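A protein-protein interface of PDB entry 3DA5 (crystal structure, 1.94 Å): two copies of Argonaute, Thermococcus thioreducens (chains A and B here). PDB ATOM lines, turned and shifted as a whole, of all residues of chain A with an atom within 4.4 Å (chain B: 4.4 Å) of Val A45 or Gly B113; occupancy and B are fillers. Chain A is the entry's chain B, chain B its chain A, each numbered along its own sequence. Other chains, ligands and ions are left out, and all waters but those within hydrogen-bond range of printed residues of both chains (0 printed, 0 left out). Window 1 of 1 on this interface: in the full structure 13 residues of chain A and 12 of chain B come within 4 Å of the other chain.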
ATOM      1  N   LEU A  34      25.689 -13.987   1.286  1.00  0.00           N
ATOM      2  CA  LEU A  34      24.945 -13.129   0.413  1.00  0.00           C
ATOM      3  C   LEU A  34      25.588 -11.739   0.366  1.00  0.00           C
ATOM      4  O   LEU A  34      26.325 -11.355   1.272  1.00  0.00           O
ATOM      5  CB  LEU A  34      23.464 -13.030   0.877  1.00  0.00           C
ATOM      6  CG  LEU A  34      22.710 -14.374   0.942  1.00  0.00           C
ATOM      7  CD1 LEU A  34      21.379 -14.118   1.737  1.00  0.00           C
ATOM      8  CD2 LEU A  34      22.439 -15.012  -0.415  1.00  0.00           C
ATOM      9  N   LEU A  35      25.327 -11.038  -0.733  1.00  0.00           N
ATOM     10  CA  LEU A  35      25.860  -9.745  -0.989  1.00  0.00           C
ATOM     11  C   LEU A  35      24.754  -8.750  -1.306  1.00  0.00           C
ATOM     12  O   LEU A  35      23.899  -8.993  -2.155  1.00  0.00           O
ATOM     13  CB  LEU A  35      26.812  -9.820  -2.214  1.00  0.00           C
ATOM     14  CG  LEU A  35      27.935 -10.846  -2.047  1.00  0.00           C
ATOM     15  CD1 LEU A  35      28.765 -10.973  -3.365  1.00  0.00           C
ATOM     16  CD2 LEU A  35      28.816 -10.424  -0.932  1.00  0.00           C
ATOM     17  N   ARG A  36      24.814  -7.616  -0.631  1.00  0.00           N
ATOM     18  CA  ARG A  36      23.856  -6.526  -0.858  1.00  0.00           C
ATOM     19  C   ARG A  36      24.555  -5.427  -1.640  1.00  0.00           C
ATOM     20  O   ARG A  36      25.582  -4.984  -1.187  1.00  0.00           O
ATOM     21  CB  ARG A  36      23.490  -5.946   0.524  1.00  0.00           C
ATOM     22  CG  ARG A  36      22.403  -4.884   0.473  1.00  0.00           C
ATOM     23  CD  ARG A  36      22.266  -4.241   1.849  1.00  0.00           C
ATOM     24  NE  ARG A  36      21.701  -5.233   2.746  1.00  0.00           N
ATOM     25  CZ  ARG A  36      22.235  -5.609   3.906  1.00  0.00           C
ATOM     26  NH1 ARG A  36      23.339  -5.035   4.398  1.00  0.00           N
ATOM     27  NH2 ARG A  36      21.624  -6.553   4.612  1.00  0.00           N
ATOM     28  N   LYS A  43      18.050  -1.943  -2.779  1.00  0.00           N
ATOM     29  CA  LYS A  43      19.057  -2.722  -2.010  1.00  0.00           C
ATOM     30  C   LYS A  43      18.940  -4.243  -2.191  1.00  0.00           C
ATOM     31  O   LYS A  43      18.756  -4.991  -1.246  1.00  0.00           O
ATOM     32  CB  LYS A  43      18.911  -2.364  -0.518  1.00  0.00           C
ATOM     33  CG  LYS A  43      19.917  -1.326  -0.011  1.00  0.00           C
ATOM     34  CD  LYS A  43      20.178  -0.162  -0.967  1.00  0.00           C
ATOM     35  CE  LYS A  43      21.003   0.918  -0.266  1.00  0.00           C
ATOM     36  NZ  LYS A  43      21.264   2.096  -1.139  1.00  0.00           N
ATOM     37  N   VAL A  44      19.068  -4.694  -3.423  1.00  0.00           N
ATOM     38  CA  VAL A  44      18.813  -6.089  -3.709  1.00  0.00           C
ATOM     39  C   VAL A  44      19.903  -6.895  -3.049  1.00  0.00           C
ATOM     40  O   VAL A  44      21.055  -6.448  -2.990  1.00  0.00           O
ATOM     41  CB  VAL A  44      18.779  -6.336  -5.170  1.00  0.00           C
ATOM     42  CG1 VAL A  44      18.415  -7.759  -5.461  1.00  0.00           C
ATOM     43  CG2 VAL A  44      17.755  -5.433  -5.776  1.00  0.00           C
ATOM     44  N   VAL A  45      19.540  -8.034  -2.486  1.00  0.00           N
ATOM     45  CA  VAL A  45      20.547  -8.949  -1.962  1.00  0.00           C
ATOM     46  C   VAL A  45      20.721 -10.026  -3.006  1.00  0.00           C
ATOM     47  O   VAL A  45      19.761 -10.365  -3.724  1.00  0.00           O
ATOM     48  CB  VAL A  45      20.186  -9.465  -0.541  1.00  0.00           C
ATOM     49  CG1 VAL A  45      21.271 -10.358  -0.014  1.00  0.00           C
ATOM     50  CG2 VAL A  45      19.938  -8.267   0.445  1.00  0.00           C
ATOM     51  N   TYR A  46      21.975 -10.499  -3.156  1.00  0.00           N
ATOM     52  CA  TYR A  46      22.362 -11.406  -4.259  1.00  0.00           C
ATOM     53  C   TYR A  46      23.071 -12.619  -3.715  1.00  0.00           C
ATOM     54  O   TYR A  46      23.833 -12.483  -2.740  1.00  0.00           O
ATOM     55  CB  TYR A  46      23.343 -10.714  -5.259  1.00  0.00           C
ATOM     56  CG  TYR A  46      22.787  -9.539  -6.018  1.00  0.00           C
ATOM     57  CD1 TYR A  46      22.305  -9.667  -7.316  1.00  0.00           C
ATOM     58  CD2 TYR A  46      22.802  -8.279  -5.460  1.00  0.00           C
ATOM     59  CE1 TYR A  46      21.786  -8.544  -7.983  1.00  0.00           C
ATOM     60  CE2 TYR A  46      22.325  -7.171  -6.128  1.00  0.00           C
ATOM     61  CZ  TYR A  46      21.791  -7.302  -7.349  1.00  0.00           C
ATOM     62  OH  TYR A  46      21.305  -6.168  -7.964  1.00  0.00           O
ATOM     63  N   PRO A 106      20.102 -12.284  -8.129  1.00  0.00           N
ATOM     64  CA  PRO A 106      19.421 -11.481  -7.119  1.00  0.00           C
ATOM     65  C   PRO A 106      18.388 -12.330  -6.387  1.00  0.00           C
ATOM     66  O   PRO A 106      17.759 -13.204  -7.009  1.00  0.00           O
ATOM     67  CB  PRO A 106      18.723 -10.392  -7.944  1.00  0.00           C
ATOM     68  CG  PRO A 106      18.441 -11.043  -9.221  1.00  0.00           C
ATOM     69  CD  PRO A 106      19.673 -11.915  -9.481  1.00  0.00           C
ATOM     70  N   LEU A 107      18.252 -12.106  -5.093  1.00  0.00           N
ATOM     71  CA  LEU A 107      17.328 -12.925  -4.303  1.00  0.00           C
ATOM     72  C   LEU A 107      15.965 -12.217  -4.395  1.00  0.00           C
ATOM     73  O   LEU A 107      15.604 -11.368  -3.579  1.00  0.00           O
ATOM     74  CB  LEU A 107      17.776 -13.093  -2.865  1.00  0.00           C
ATOM     75  CG  LEU A 107      18.853 -14.127  -2.473  1.00  0.00           C
ATOM     76  CD1 LEU A 107      18.639 -14.437  -1.016  1.00  0.00           C
ATOM     77  CD2 LEU A 107      18.853 -15.419  -3.298  1.00  0.00           C
ATOM     78  N   VAL A 126      26.355 -10.384   3.485  1.00  0.00           N
ATOM     79  CA  VAL A 126      25.233 -10.696   4.391  1.00  0.00           C
ATOM     80  C   VAL A 126      25.247 -12.215   4.649  1.00  0.00           C
ATOM     81  O   VAL A 126      25.306 -12.953   3.672  1.00  0.00           O
ATOM     82  CB  VAL A 126      23.869 -10.380   3.726  1.00  0.00           C
ATOM     83  CG1 VAL A 126      22.743 -10.422   4.780  1.00  0.00           C
ATOM     84  CG2 VAL A 126      23.871  -9.028   2.946  1.00  0.00           C
ATOM     85  N   PRO B 106       9.192 -11.978   1.697  1.00  0.00           N
ATOM     86  CA  PRO B 106       8.803 -11.226   2.841  1.00  0.00           C
ATOM     87  C   PRO B 106       7.743 -10.193   2.469  1.00  0.00           C
ATOM     88  O   PRO B 106       7.638  -9.783   1.296  1.00  0.00           O
ATOM     89  CB  PRO B 106      10.092 -10.545   3.249  1.00  0.00           C
ATOM     90  CG  PRO B 106      10.867 -10.491   2.063  1.00  0.00           C
ATOM     91  CD  PRO B 106      10.585 -11.665   1.317  1.00  0.00           C
ATOM     92  N   HIS B 110      13.649  -6.935   3.836  1.00  0.00           N
ATOM     93  CA  HIS B 110      14.200  -8.025   4.642  1.00  0.00           C
ATOM     94  C   HIS B 110      15.736  -8.066   4.468  1.00  0.00           C
ATOM     95  O   HIS B 110      16.227  -7.909   3.341  1.00  0.00           O
ATOM     96  CB  HIS B 110      13.624  -9.328   4.058  1.00  0.00           C
ATOM     97  CG  HIS B 110      13.772 -10.539   4.928  1.00  0.00           C
ATOM     98  ND1 HIS B 110      14.202 -11.752   4.438  1.00  0.00           N
ATOM     99  CD2 HIS B 110      13.498 -10.740   6.241  1.00  0.00           C
ATOM    100  CE1 HIS B 110      14.224 -12.643   5.426  1.00  0.00           C
ATOM    101  NE2 HIS B 110      13.794 -12.055   6.527  1.00  0.00           N
ATOM    102  N   ASN B 111      16.484  -8.365   5.541  1.00  0.00           N
ATOM    103  CA  ASN B 111      17.948  -8.465   5.435  1.00  0.00           C
ATOM    104  C   ASN B 111      18.471  -9.563   4.522  1.00  0.00           C
ATOM    105  O   ASN B 111      19.519  -9.397   3.941  1.00  0.00           O
ATOM    106  CB  ASN B 111      18.606  -8.571   6.813  1.00  0.00           C
ATOM    107  CG  ASN B 111      18.500  -7.264   7.597  1.00  0.00           C
ATOM    108  OD1 ASN B 111      18.558  -7.270   8.826  1.00  0.00           O
ATOM    109  ND2 ASN B 111      18.296  -6.142   6.888  1.00  0.00           N
ATOM    110  N   ARG B 112      17.725 -10.646   4.348  1.00  0.00           N
ATOM    111  CA  ARG B 112      18.138 -11.733   3.451  1.00  0.00           C
ATOM    112  C   ARG B 112      17.598 -11.608   2.062  1.00  0.00           C
ATOM    113  O   ARG B 112      17.641 -12.574   1.292  1.00  0.00           O
ATOM    114  CB  ARG B 112      17.710 -13.091   4.030  1.00  0.00           C
ATOM    115  CG  ARG B 112      18.597 -13.559   5.184  1.00  0.00           C
ATOM    116  CD  ARG B 112      19.808 -14.337   4.647  1.00  0.00           C
ATOM    117  NE  ARG B 112      20.865 -14.522   5.628  1.00  0.00           N
ATOM    118  CZ  ARG B 112      21.956 -15.262   5.415  1.00  0.00           C
ATOM    119  NH1 ARG B 112      22.890 -15.377   6.365  1.00  0.00           N
ATOM    120  NH2 ARG B 112      22.121 -15.905   4.262  1.00  0.00           N
ATOM    121  N   GLY B 113      17.071 -10.444   1.721  1.00  0.00           N
ATOM    122  CA  GLY B 113      16.562 -10.244   0.365  1.00  0.00           C
ATOM    123  C   GLY B 113      15.104 -10.605   0.270  1.00  0.00           C
ATOM    124  O   GLY B 113      14.441 -10.801   1.266  1.00  0.00           O
ATOM    125  N   ASP B 114      14.621 -10.706  -0.948  1.00  0.00           N
ATOM    126  CA  ASP B 114      13.208 -10.784  -1.231  1.00  0.00           C
ATOM    127  C   ASP B 114      12.754 -12.145  -1.734  1.00  0.00           C
ATOM    128  O   ASP B 114      11.701 -12.275  -2.346  1.00  0.00           O
ATOM    129  CB  ASP B 114      12.859  -9.666  -2.205  1.00  0.00           C
ATOM    130  CG  ASP B 114      12.686  -8.306  -1.484  1.00  0.00           C
ATOM    131  OD1 ASP B 114      13.129  -8.138  -0.314  1.00  0.00           O
ATOM    132  OD2 ASP B 114      12.057  -7.417  -2.072  1.00  0.00           O
ATOM    133  N   LEU B 115      13.539 -13.166  -1.417  1.00  0.00           N
ATOM    134  CA  LEU B 115      13.192 -14.545  -1.724  1.00  0.00           C
ATOM    135  C   LEU B 115      13.801 -15.477  -0.714  1.00  0.00           C
ATOM    136  O   LEU B 115      15.033 -15.473  -0.536  1.00  0.00           O
ATOM    137  CB  LEU B 115      13.731 -14.965  -3.059  1.00  0.00           C
ATOM    138  CG  LEU B 115      13.785 -16.479  -3.343  1.00  0.00           C
ATOM    139  CD1 LEU B 115      12.395 -17.021  -3.597  1.00  0.00           C
ATOM    140  CD2 LEU B 115      14.738 -16.759  -4.562  1.00  0.00           C
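The backbone NH (N) of Asp B114 lies within hydrogen-bond range of the backbone carbonyl oxygen (O) of Leu A107, at 2.9 Å.
The backbone carbonyl oxygen (O) of Leu A107 sits at hydrogen-bond distance from the backbone NH (N) of Leu B115 (3.5 Å).
ND1 of His B110 sits close to O of Gly B113, 3.3 Å away.
The backbone carbonyl oxygen (O) of Leu A34 sits at hydrogen-bond distance from the backbone NH (N) of Val A126 (2.4 Å).
The backbone NH (N) of Leu A107 is in hydrogen-bond range of the backbone carbonyl oxygen (O) of Val A45 (2.7 Å).
Among the printed residues, merely in contact across the chains: Leu A107 with Arg B112 (3.1 Å), Leu A34 with Arg B112 (3.2 Å), Val A126 with Asn B111 (3.5 Å), Arg A36 with Asn B111 (3.6 Å), Val A45 with Asn B111 (3.7 Å), Val A45 with Gly B113 (3.8 Å) and Leu A107 with Gly B113 (3.96 Å).
Of the printed residues of chain B, Arg A36 touches Asn B111.
Val A45 touches two residues of chain B.
Tyr A46 touches none of the printed residues of chain B.
Printed residues of chain B within 4 Å of Val A126: Asn B111 (3.5 Å).
Of the printed residues of chain A, Arg B112 touches Leu A34 (3.2 Å) and Leu A107 (3.1 Å).
Of chain A, only Val A45 and Leu A107 come within 4 Å of Gly B113.
Of the printed residues of chain A, Asp B114 touches Leu A107 (2.9 Å).
Of the printed residues of chain A, Leu B115 touches Leu A107.
The nearest residue of chain B that does not touch Val A45 is Arg B112 (4.3 Å).
Hydrophobic or aromatic side chains of chain A within 4 Å of the printed part of chain B: Leu A34, Val A45, Leu A107 and Val A126.
Printed residues of chain B that touch a printed residue of chain A: Asn B111, Arg B112, Gly B113, Asp B114 and Leu B115.
Hydrophobic or aromatic side chains of chain B within 4 Å of the printed part of chain A: Leu B115.
Among the printed residues, 9 pairs touch across the chains.
Among the printed residues, no Asp or Glu carboxylate lies within 4 Å of a Lys or Arg side-chain nitrogen of the other chain.
Position printed for both chains: 106.
Of the 9 pairs that touch across the chains among the printed residues, none has its exchanged pair printed and touching as well.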
